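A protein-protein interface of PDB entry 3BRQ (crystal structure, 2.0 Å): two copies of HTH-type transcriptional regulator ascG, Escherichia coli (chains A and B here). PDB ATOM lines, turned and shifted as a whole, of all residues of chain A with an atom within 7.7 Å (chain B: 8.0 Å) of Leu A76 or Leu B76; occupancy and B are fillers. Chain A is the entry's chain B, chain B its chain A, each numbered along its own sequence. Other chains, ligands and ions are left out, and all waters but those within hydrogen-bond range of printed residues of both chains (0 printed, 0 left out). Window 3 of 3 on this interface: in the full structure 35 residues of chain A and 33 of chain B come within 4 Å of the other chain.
Among the printed residues, pairs that only touch across the chains: Leu A54 with Ala B57, Leu A55 with Leu B56, Leu A55 with Tyr B72, Leu A55 with Leu B73, Leu A55 with Leu B76, Ala A57 with Leu B54, Tyr A72 with Gln B53, Tyr A72 with Leu B55, Leu A73 with Leu B55, Leu A76 with Leu B55 and Leu A76 with Leu B76.
The backbone NH of Thr B21 is in hydrogen-bond range of the side-chain carboxylate of Asp B79 (2.7 Å). The backbone carbonyl oxygen of Leu B73 sits at hydrogen-bond distance from the backbone NH of Cys B78, at 3.0 Å. N of Thr A21 is in hydrogen-bond range of OD2 of Asp A79. The backbone NH (N) of Cys A78 lies within hydrogen-bond range of the backbone carbonyl oxygen (O) of Leu A73, 3.1 Å away.
Of chain B, only Leu B55 (3.7 Å) and Leu B76 (3.7 Å) come within 4 Å of Leu A76. Of chain A, only Leu A55 (3.4 Å) and Leu A76 (3.7 Å) come within 4 Å of Leu B76. Of the printed residues of chain A, Leu B54 touches Ala A57. Printed residues of chain A within 4 Å of Leu B73: Leu A55 (3.8 Å). Of the printed residues of chain B, Leu A73 touches Leu B55. Of the printed residues of chain B, Thr A21 touches Tyr B72 (2.5 Å). Of the printed residues of chain B, Leu A54 touches Ala B57 (3.9 Å). Asp B79 touches none of the printed residues of chain A. Gln B71 touches none of the printed residues of chain A.
Thr A21 touches Tyr B72, and with the chains exchanged Tyr A72 touches Thr B21. Leu A54 touches Ala B57, and with the chains exchanged Ala A57 touches Leu B54. Leu A55 touches Tyr B72, and with the chains exchanged Tyr A72 touches Leu B55. Leu A55 touches Leu B73, and with the chains exchanged Leu A73 touches Leu B55. Positions printed for both chains: 21, 54, 55, 57, 69, 70, 71, 72, 73, 74, 75, 76, 77, 78 and 79. Of the 13 pairs that touch across the chains among the printed residues, 11 have their exchanged pair printed and touching as well.
The side-chain hydroxyl of Thr B21 lies within hydrogen-bond range of the side-chain hydroxyl of Tyr A72. OH of Tyr B72 sits at hydrogen-bond distance from OG1 of Thr A21 (2.5 Å).
Of the 18 printed residues of chain B, 9 touch a printed residue of chain A. Of the 15 printed residues of chain A, 7 touch a printed residue of chain B. Hydrophobic or aromatic side chains of chain A that line the printed part of chain B: Leu A55, Tyr A72, Leu A73 and Leu A76.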
ATOM      1  N   THR A  21     -18.740 -23.436  29.603  1.00  0.00           N
ATOM      2  CA  THR A  21     -19.208 -22.842  28.365  1.00  0.00           C
ATOM      3  C   THR A  21     -18.143 -21.876  27.861  1.00  0.00           C
ATOM      4  O   THR A  21     -17.604 -21.108  28.661  1.00  0.00           O
ATOM      5  CB  THR A  21     -20.549 -22.143  28.631  1.00  0.00           C
ATOM      6  OG1 THR A  21     -21.535 -23.137  28.950  1.00  0.00           O
ATOM      7  CG2 THR A  21     -21.016 -21.345  27.431  1.00  0.00           C
ATOM      8  N   LEU A  54     -20.658 -24.169  23.522  1.00  0.00           N
ATOM      9  CA  LEU A  54     -20.261 -22.973  22.833  1.00  0.00           C
ATOM     10  C   LEU A  54     -21.460 -22.022  22.798  1.00  0.00           C
ATOM     11  O   LEU A  54     -22.590 -22.464  22.492  1.00  0.00           O
ATOM     12  CB  LEU A  54     -19.885 -23.351  21.406  1.00  0.00           C
ATOM     13  CG  LEU A  54     -19.316 -22.232  20.542  1.00  0.00           C
ATOM     14  CD1 LEU A  54     -17.867 -22.090  20.873  1.00  0.00           C
ATOM     15  CD2 LEU A  54     -19.501 -22.600  19.103  1.00  0.00           C
ATOM     16  N   LEU A  55     -21.202 -20.747  23.091  1.00  0.00           N
ATOM     17  CA  LEU A  55     -22.189 -19.661  22.943  1.00  0.00           C
ATOM     18  C   LEU A  55     -21.581 -18.542  22.088  1.00  0.00           C
ATOM     19  O   LEU A  55     -20.481 -18.098  22.381  1.00  0.00           O
ATOM     20  CB  LEU A  55     -22.566 -19.057  24.311  1.00  0.00           C
ATOM     21  CG  LEU A  55     -23.663 -19.807  25.094  1.00  0.00           C
ATOM     22  CD1 LEU A  55     -24.024 -19.052  26.382  1.00  0.00           C
ATOM     23  CD2 LEU A  55     -24.903 -20.034  24.213  1.00  0.00           C
ATOM     24  N   ALA A  57     -22.247 -14.620  20.917  1.00  0.00           N
ATOM     25  CA  ALA A  57     -23.094 -13.448  21.013  1.00  0.00           C
ATOM     26  C   ALA A  57     -22.740 -12.448  19.899  1.00  0.00           C
ATOM     27  O   ALA A  57     -21.562 -12.180  19.621  1.00  0.00           O
ATOM     28  CB  ALA A  57     -22.961 -12.790  22.448  1.00  0.00           C
ATOM     29  N   ALA A  69     -21.577  -7.026  24.855  1.00  0.00           N
ATOM     30  CA  ALA A  69     -21.755  -8.471  24.471  1.00  0.00           C
ATOM     31  C   ALA A  69     -20.833  -9.371  25.321  1.00  0.00           C
ATOM     32  O   ALA A  69     -21.197 -10.483  25.712  1.00  0.00           O
ATOM     33  CB  ALA A  69     -21.430  -8.646  22.990  1.00  0.00           C
ATOM     34  N   ILE A  70     -19.640  -8.841  25.665  1.00  0.00           N
ATOM     35  CA  ILE A  70     -18.727  -9.541  26.543  1.00  0.00           C
ATOM     36  C   ILE A  70     -19.384  -9.711  27.920  1.00  0.00           C
ATOM     37  O   ILE A  70     -19.516 -10.823  28.399  1.00  0.00           O
ATOM     38  CB  ILE A  70     -17.311  -8.824  26.641  1.00  0.00           C
ATOM     39  CG1 ILE A  70     -16.535  -8.996  25.314  1.00  0.00           C
ATOM     40  CG2 ILE A  70     -16.482  -9.360  27.895  1.00  0.00           C
ATOM     41  CD1 ILE A  70     -15.409  -7.946  25.080  1.00  0.00           C
ATOM     42  N   GLN A  71     -19.809  -8.608  28.540  1.00  0.00           N
ATOM     43  CA  GLN A  71     -20.547  -8.658  29.816  1.00  0.00           C
ATOM     44  C   GLN A  71     -21.780  -9.515  29.799  1.00  0.00           C
ATOM     45  O   GLN A  71     -22.063 -10.192  30.789  1.00  0.00           O
ATOM     46  CB  GLN A  71     -20.970  -7.268  30.263  1.00  0.00           C
ATOM     47  CG  GLN A  71     -21.399  -7.251  31.724  1.00  0.00           C
ATOM     48  CD  GLN A  71     -20.278  -7.714  32.667  1.00  0.00           C
ATOM     49  OE1 GLN A  71     -19.174  -7.161  32.642  1.00  0.00           O
ATOM     50  NE2 GLN A  71     -20.567  -8.719  33.510  1.00  0.00           N
ATOM     51  N   TYR A  72     -22.558  -9.422  28.725  1.00  0.00           N
ATOM     52  CA  TYR A  72     -23.711 -10.280  28.547  1.00  0.00           C
ATOM     53  C   TYR A  72     -23.296 -11.726  28.720  1.00  0.00           C
ATOM     54  O   TYR A  72     -23.908 -12.447  29.494  1.00  0.00           O
ATOM     55  CB  TYR A  72     -24.354 -10.053  27.181  1.00  0.00           C
ATOM     56  CG  TYR A  72     -25.563 -10.926  26.881  1.00  0.00           C
ATOM     57  CD1 TYR A  72     -26.710 -10.883  27.693  1.00  0.00           C
ATOM     58  CD2 TYR A  72     -25.561 -11.799  25.803  1.00  0.00           C
ATOM     59  CE1 TYR A  72     -27.829 -11.690  27.419  1.00  0.00           C
ATOM     60  CE2 TYR A  72     -26.693 -12.616  25.522  1.00  0.00           C
ATOM     61  CZ  TYR A  72     -27.817 -12.546  26.342  1.00  0.00           C
ATOM     62  OH  TYR A  72     -28.936 -13.358  26.089  1.00  0.00           O
ATOM     63  N   LEU A  73     -22.279 -12.169  28.000  1.00  0.00           N
ATOM     64  CA  LEU A  73     -21.880 -13.581  28.078  1.00  0.00           C
ATOM     65  C   LEU A  73     -21.404 -14.026  29.438  1.00  0.00           C
ATOM     66  O   LEU A  73     -21.719 -15.126  29.868  1.00  0.00           O
ATOM     67  CB  LEU A  73     -20.842 -13.964  27.010  1.00  0.00           C
ATOM     68  CG  LEU A  73     -21.285 -14.065  25.550  1.00  0.00           C
ATOM     69  CD1 LEU A  73     -20.081 -14.417  24.703  1.00  0.00           C
ATOM     70  CD2 LEU A  73     -22.429 -15.106  25.326  1.00  0.00           C
ATOM     71  N   LEU A  74     -20.668 -13.169  30.115  1.00  0.00           N
ATOM     72  CA  LEU A  74     -20.292 -13.443  31.495  1.00  0.00           C
ATOM     73  C   LEU A  74     -21.495 -13.607  32.453  1.00  0.00           C
ATOM     74  O   LEU A  74     -21.507 -14.510  33.323  1.00  0.00           O
ATOM     75  CB  LEU A  74     -19.378 -12.328  31.983  1.00  0.00           C
ATOM     76  CG  LEU A  74     -18.111 -12.349  31.161  1.00  0.00           C
ATOM     77  CD1 LEU A  74     -17.153 -11.269  31.710  1.00  0.00           C
ATOM     78  CD2 LEU A  74     -17.468 -13.787  31.207  1.00  0.00           C
ATOM     79  N   ASP A  75     -22.528 -12.780  32.237  1.00  0.00           N
ATOM     80  CA  ASP A  75     -23.715 -12.799  33.058  1.00  0.00           C
ATOM     81  C   ASP A  75     -24.534 -14.032  32.663  1.00  0.00           C
ATOM     82  O   ASP A  75     -25.518 -14.371  33.337  1.00  0.00           O
ATOM     83  CB  ASP A  75     -24.540 -11.554  32.781  1.00  0.00           C
ATOM     84  CG  ASP A  75     -23.887 -10.291  33.309  1.00  0.00           C
ATOM     85  OD1 ASP A  75     -22.903 -10.403  34.035  1.00  0.00           O
ATOM     86  OD2 ASP A  75     -24.359  -9.191  33.009  1.00  0.00           O
ATOM     87  N   LEU A  76     -24.176 -14.678  31.564  1.00  0.00           N
ATOM     88  CA  LEU A  76     -24.781 -15.985  31.280  1.00  0.00           C
ATOM     89  C   LEU A  76     -23.886 -17.081  31.869  1.00  0.00           C
ATOM     90  O   LEU A  76     -24.162 -18.264  31.704  1.00  0.00           O
ATOM     91  CB  LEU A  76     -25.000 -16.173  29.788  1.00  0.00           C
ATOM     92  CG  LEU A  76     -25.921 -15.126  29.155  1.00  0.00           C
ATOM     93  CD1 LEU A  76     -25.989 -15.382  27.651  1.00  0.00           C
ATOM     94  CD2 LEU A  76     -27.299 -15.166  29.808  1.00  0.00           C
ATOM     95  N   ARG A  77     -22.852 -16.671  32.598  1.00  0.00           N
ATOM     96  CA  ARG A  77     -21.876 -17.600  33.175  1.00  0.00           C
ATOM     97  C   ARG A  77     -21.095 -18.406  32.137  1.00  0.00           C
ATOM     98  O   ARG A  77     -20.822 -19.586  32.347  1.00  0.00           O
ATOM     99  CB  ARG A  77     -22.496 -18.567  34.212  1.00  0.00           C
ATOM    100  CG  ARG A  77     -21.592 -18.789  35.441  1.00  0.00           C
ATOM    101  CD  ARG A  77     -21.942 -20.065  36.242  1.00  0.00           C
ATOM    102  NE  ARG A  77     -23.347 -20.139  36.627  1.00  0.00           N
ATOM    103  CZ  ARG A  77     -23.790 -20.594  37.808  1.00  0.00           C
ATOM    104  NH1 ARG A  77     -22.930 -20.992  38.755  1.00  0.00           N
ATOM    105  NH2 ARG A  77     -25.101 -20.641  38.051  1.00  0.00           N
ATOM    106  N   CYS A  78     -20.711 -17.773  31.033  1.00  0.00           N
ATOM    107  CA  CYS A  78     -19.557 -18.267  30.276  1.00  0.00           C
ATOM    108  C   CYS A  78     -18.301 -18.263  31.138  1.00  0.00           C
ATOM    109  O   CYS A  78     -18.014 -17.297  31.846  1.00  0.00           O
ATOM    110  CB  CYS A  78     -19.312 -17.453  29.006  1.00  0.00           C
ATOM    111  SG  CYS A  78     -20.616 -17.724  27.824  1.00  0.00           S
ATOM    112  N   ASP A  79     -17.543 -19.347  31.047  1.00  0.00           N
ATOM    113  CA  ASP A  79     -16.335 -19.554  31.864  1.00  0.00           C
ATOM    114  C   ASP A  79     -15.074 -18.914  31.252  1.00  0.00           C
ATOM    115  O   ASP A  79     -14.160 -18.562  31.971  1.00  0.00           O
ATOM    116  CB  ASP A  79     -16.148 -21.054  32.078  1.00  0.00           C
ATOM    117  CG  ASP A  79     -17.397 -21.707  32.696  1.00  0.00           C
ATOM    118  OD1 ASP A  79     -17.529 -21.613  33.921  1.00  0.00           O
ATOM    119  OD2 ASP A  79     -18.272 -22.239  31.965  1.00  0.00           O
ATOM    120  N   THR B  21     -33.738 -11.566  24.098  1.00  0.00           N
ATOM    121  CA  THR B  21     -32.747 -12.309  23.351  1.00  0.00           C
ATOM    122  C   THR B  21     -33.435 -13.317  22.422  1.00  0.00           C
ATOM    123  O   THR B  21     -34.366 -14.022  22.820  1.00  0.00           O
ATOM    124  CB  THR B  21     -31.767 -13.032  24.306  1.00  0.00           C
ATOM    125  OG1 THR B  21     -31.004 -12.074  25.006  1.00  0.00           O
ATOM    126  CG2 THR B  21     -30.757 -13.899  23.528  1.00  0.00           C
ATOM    127  N   GLN B  53     -31.025  -8.965  21.117  1.00  0.00           N
ATOM    128  CA  GLN B  53     -29.721  -9.633  21.156  1.00  0.00           C
ATOM    129  C   GLN B  53     -29.843 -10.995  20.502  1.00  0.00           C
ATOM    130  O   GLN B  53     -30.756 -11.732  20.850  1.00  0.00           O
ATOM    131  CB  GLN B  53     -29.282  -9.794  22.627  1.00  0.00           C
ATOM    132  CG  GLN B  53     -27.856 -10.422  22.930  1.00  0.00           C
ATOM    133  CD  GLN B  53     -26.647  -9.754  22.237  1.00  0.00           C
ATOM    134  OE1 GLN B  53     -26.038 -10.327  21.312  1.00  0.00           O
ATOM    135  NE2 GLN B  53     -26.254  -8.603  22.725  1.00  0.00           N
ATOM    136  N   LEU B  54     -28.965 -11.314  19.535  1.00  0.00           N
ATOM    137  CA  LEU B  54     -28.832 -12.694  19.024  1.00  0.00           C
ATOM    138  C   LEU B  54     -27.754 -13.490  19.794  1.00  0.00           C
ATOM    139  O   LEU B  54     -26.619 -12.999  20.070  1.00  0.00           O
ATOM    140  CB  LEU B  54     -28.592 -12.724  17.508  1.00  0.00           C
ATOM    141  CG  LEU B  54     -28.693 -14.057  16.734  1.00  0.00           C
ATOM    142  CD1 LEU B  54     -30.127 -14.596  16.771  1.00  0.00           C
ATOM    143  CD2 LEU B  54     -28.282 -13.906  15.295  1.00  0.00           C
ATOM    144  N   LEU B  55     -28.126 -14.707  20.157  1.00  0.00           N
ATOM    145  CA  LEU B  55     -27.231 -15.644  20.786  1.00  0.00           C
ATOM    146  C   LEU B  55     -27.318 -16.960  20.009  1.00  0.00           C
ATOM    147  O   LEU B  55     -28.421 -17.410  19.717  1.00  0.00           O
ATOM    148  CB  LEU B  55     -27.712 -15.880  22.233  1.00  0.00           C
ATOM    149  CG  LEU B  55     -26.832 -16.615  23.225  1.00  0.00           C
ATOM    150  CD1 LEU B  55     -25.558 -15.824  23.467  1.00  0.00           C
ATOM    151  CD2 LEU B  55     -27.610 -16.744  24.590  1.00  0.00           C
ATOM    152  N   LEU B  56     -26.183 -17.565  19.654  1.00  0.00           N
ATOM    153  CA  LEU B  56     -26.247 -18.818  18.900  1.00  0.00           C
ATOM    154  C   LEU B  56     -25.646 -19.930  19.735  1.00  0.00           C
ATOM    155  O   LEU B  56     -24.633 -19.722  20.375  1.00  0.00           O
ATOM    156  CB  LEU B  56     -25.536 -18.702  17.525  1.00  0.00           C
ATOM    157  CG  LEU B  56     -25.271 -20.034  16.774  1.00  0.00           C
ATOM    158  CD1 LEU B  56     -25.309 -19.877  15.303  1.00  0.00           C
ATOM    159  CD2 LEU B  56     -23.939 -20.570  17.135  1.00  0.00           C
ATOM    160  N   ALA B  57     -26.273 -21.106  19.672  1.00  0.00           N
ATOM    161  CA  ALA B  57     -25.764 -22.362  20.265  1.00  0.00           C
ATOM    162  C   ALA B  57     -25.543 -23.449  19.203  1.00  0.00           C
ATOM    163  O   ALA B  57     -26.202 -23.462  18.175  1.00  0.00           O
ATOM    164  CB  ALA B  57     -26.731 -22.878  21.317  1.00  0.00           C
ATOM    165  N   ALA B  69     -29.522 -28.087  23.012  1.00  0.00           N
ATOM    166  CA  ALA B  69     -29.132 -26.699  22.616  1.00  0.00           C
ATOM    167  C   ALA B  69     -30.280 -25.729  22.847  1.00  0.00           C
ATOM    168  O   ALA B  69     -30.107 -24.638  23.451  1.00  0.00           O
ATOM    169  CB  ALA B  69     -28.756 -26.667  21.172  1.00  0.00           C
ATOM    170  N   ILE B  70     -31.457 -26.137  22.362  1.00  0.00           N
ATOM    171  CA  ILE B  70     -32.665 -25.378  22.610  1.00  0.00           C
ATOM    172  C   ILE B  70     -32.945 -25.170  24.102  1.00  0.00           C
ATOM    173  O   ILE B  70     -33.208 -24.047  24.517  1.00  0.00           O
ATOM    174  CB  ILE B  70     -33.882 -26.079  21.956  1.00  0.00           C
ATOM    175  CG1 ILE B  70     -33.707 -26.071  20.446  1.00  0.00           C
ATOM    176  CG2 ILE B  70     -35.231 -25.433  22.397  1.00  0.00           C
ATOM    177  CD1 ILE B  70     -34.698 -27.064  19.705  1.00  0.00           C
ATOM    178  N   GLN B  71     -32.920 -26.243  24.894  1.00  0.00           N
ATOM    179  CA  GLN B  71     -33.141 -26.136  26.331  1.00  0.00           C
ATOM    180  C   GLN B  71     -32.093 -25.215  27.000  1.00  0.00           C
ATOM    181  O   GLN B  71     -32.423 -24.435  27.894  1.00  0.00           O
ATOM    182  CB  GLN B  71     -33.060 -27.528  26.950  1.00  0.00           C
ATOM    183  CG  GLN B  71     -33.674 -27.673  28.358  1.00  0.00           C
ATOM    184  CD  GLN B  71     -35.039 -26.998  28.457  1.00  0.00           C
ATOM    185  OE1 GLN B  71     -35.972 -27.342  27.722  1.00  0.00           O
ATOM    186  NE2 GLN B  71     -35.129 -25.963  29.316  1.00  0.00           N
ATOM    187  N   TYR B  72     -30.846 -25.351  26.576  1.00  0.00           N
ATOM    188  CA  TYR B  72     -29.752 -24.565  27.119  1.00  0.00           C
ATOM    189  C   TYR B  72     -30.112 -23.095  26.973  1.00  0.00           C
ATOM    190  O   TYR B  72     -30.278 -22.417  27.964  1.00  0.00           O
ATOM    191  CB  TYR B  72     -28.424 -24.901  26.412  1.00  0.00           C
ATOM    192  CG  TYR B  72     -27.217 -24.206  27.016  1.00  0.00           C
ATOM    193  CD1 TYR B  72     -27.121 -24.037  28.372  1.00  0.00           C
ATOM    194  CD2 TYR B  72     -26.171 -23.752  26.222  1.00  0.00           C
ATOM    195  CE1 TYR B  72     -26.014 -23.437  28.958  1.00  0.00           C
ATOM    196  CE2 TYR B  72     -25.043 -23.125  26.795  1.00  0.00           C
ATOM    197  CZ  TYR B  72     -24.990 -22.980  28.174  1.00  0.00           C
ATOM    198  OH  TYR B  72     -23.941 -22.364  28.819  1.00  0.00           O
ATOM    199  N   LEU B  73     -30.361 -22.657  25.740  1.00  0.00           N
ATOM    200  CA  LEU B  73     -30.757 -21.250  25.458  1.00  0.00           C
ATOM    201  C   LEU B  73     -31.977 -20.730  26.226  1.00  0.00           C
ATOM    202  O   LEU B  73     -31.965 -19.591  26.697  1.00  0.00           O
ATOM    203  CB  LEU B  73     -30.917 -20.986  23.959  1.00  0.00           C
ATOM    204  CG  LEU B  73     -29.683 -21.077  23.070  1.00  0.00           C
ATOM    205  CD1 LEU B  73     -30.132 -20.992  21.610  1.00  0.00           C
ATOM    206  CD2 LEU B  73     -28.648 -19.978  23.379  1.00  0.00           C
ATOM    207  N   LEU B  74     -33.004 -21.550  26.345  1.00  0.00           N
ATOM    208  CA  LEU B  74     -34.147 -21.278  27.224  1.00  0.00           C
ATOM    209  C   LEU B  74     -33.780 -21.077  28.701  1.00  0.00           C
ATOM    210  O   LEU B  74     -34.316 -20.198  29.362  1.00  0.00           O
ATOM    211  CB  LEU B  74     -35.164 -22.446  27.123  1.00  0.00           C
ATOM    212  CG  LEU B  74     -35.833 -22.380  25.748  1.00  0.00           C
ATOM    213  CD1 LEU B  74     -36.789 -23.526  25.523  1.00  0.00           C
ATOM    214  CD2 LEU B  74     -36.562 -21.006  25.523  1.00  0.00           C
ATOM    215  N   ASP B  75     -32.908 -21.933  29.221  1.00  0.00           N
ATOM    216  CA  ASP B  75     -32.498 -21.841  30.609  1.00  0.00           C
ATOM    217  C   ASP B  75     -31.571 -20.631  30.821  1.00  0.00           C
ATOM    218  O   ASP B  75     -31.372 -20.213  31.941  1.00  0.00           O
ATOM    219  CB  ASP B  75     -31.825 -23.138  31.071  1.00  0.00           C
ATOM    220  CG  ASP B  75     -32.793 -24.370  31.077  1.00  0.00           C
ATOM    221  OD1 ASP B  75     -34.039 -24.230  31.056  1.00  0.00           O
ATOM    222  OD2 ASP B  75     -32.292 -25.522  31.088  1.00  0.00           O
ATOM    223  N   LEU B  76     -30.983 -20.110  29.746  1.00  0.00           N
ATOM    224  CA  LEU B  76     -30.241 -18.859  29.780  1.00  0.00           C
ATOM    225  C   LEU B  76     -31.195 -17.712  29.576  1.00  0.00           C
ATOM    226  O   LEU B  76     -30.759 -16.550  29.426  1.00  0.00           O
ATOM    227  CB  LEU B  76     -29.172 -18.797  28.681  1.00  0.00           C
ATOM    228  CG  LEU B  76     -28.096 -19.868  28.752  1.00  0.00           C
ATOM    229  CD1 LEU B  76     -27.126 -19.686  27.635  1.00  0.00           C
ATOM    230  CD2 LEU B  76     -27.399 -19.876  30.083  1.00  0.00           C
ATOM    231  N   ARG B  77     -32.490 -18.039  29.518  1.00  0.00           N
ATOM    232  CA  ARG B  77     -33.569 -17.031  29.436  1.00  0.00           C
ATOM    233  C   ARG B  77     -33.652 -16.261  28.096  1.00  0.00           C
ATOM    234  O   ARG B  77     -34.062 -15.081  28.048  1.00  0.00           O
ATOM    235  CB  ARG B  77     -33.515 -16.060  30.629  1.00  0.00           C
ATOM    236  CG  ARG B  77     -33.453 -16.760  31.979  1.00  0.00           C
ATOM    237  CD  ARG B  77     -34.181 -15.999  33.109  1.00  0.00           C
ATOM    238  NE  ARG B  77     -35.614 -15.754  32.864  1.00  0.00           N
ATOM    239  CZ  ARG B  77     -36.359 -14.858  33.527  1.00  0.00           C
ATOM    240  NH1 ARG B  77     -35.826 -14.079  34.487  1.00  0.00           N
ATOM    241  NH2 ARG B  77     -37.644 -14.724  33.216  1.00  0.00           N
ATOM    242  N   CYS B  78     -33.285 -16.925  27.006  1.00  0.00           N
ATOM    243  CA  CYS B  78     -33.668 -16.433  25.684  1.00  0.00           C
ATOM    244  C   CYS B  78     -35.174 -16.378  25.634  1.00  0.00           C
ATOM    245  O   CYS B  78     -35.873 -17.250  26.158  1.00  0.00           O
ATOM    246  CB  CYS B  78     -33.129 -17.331  24.563  1.00  0.00           C
ATOM    247  SG  CYS B  78     -31.350 -17.152  24.356  1.00  0.00           S
ATOM    248  N   ASP B  79     -35.677 -15.372  24.957  1.00  0.00           N
ATOM    249  CA  ASP B  79     -37.098 -15.135  24.919  1.00  0.00           C
ATOM    250  C   ASP B  79     -37.801 -15.943  23.824  1.00  0.00           C
ATOM    251  O   ASP B  79     -38.965 -16.244  23.937  1.00  0.00           O
ATOM    252  CB  ASP B  79     -37.316 -13.631  24.813  1.00  0.00           C
ATOM    253  CG  ASP B  79     -36.691 -12.891  26.007  1.00  0.00           C
ATOM    254  OD1 ASP B  79     -37.319 -12.882  27.071  1.00  0.00           O
ATOM    255  OD2 ASP B  79     -35.539 -12.427  25.937  1.00  0.00           O
ATOM    256  N   GLN B 102     -42.425 -20.221  25.344  1.00  0.00           N
ATOM    257  CA  GLN B 102     -41.596 -19.366  24.500  1.00  0.00           C
ATOM    258  C   GLN B 102     -41.769 -19.743  23.003  1.00  0.00           C
ATOM    259  O   GLN B 102     -41.833 -20.929  22.666  1.00  0.00           O
ATOM    260  CB  GLN B 102     -40.116 -19.392  24.946  1.00  0.00           C
ATOM    261  CG  GLN B 102     -39.896 -18.996  26.419  1.00  0.00           C
ATOM    262  CD  GLN B 102     -39.661 -20.205  27.319  1.00  0.00           C
ATOM    263  OE1 GLN B 102     -40.217 -21.281  27.091  1.00  0.00           O
ATOM    264  NE2 GLN B 102     -38.795 -20.038  28.340  1.00  0.00           N
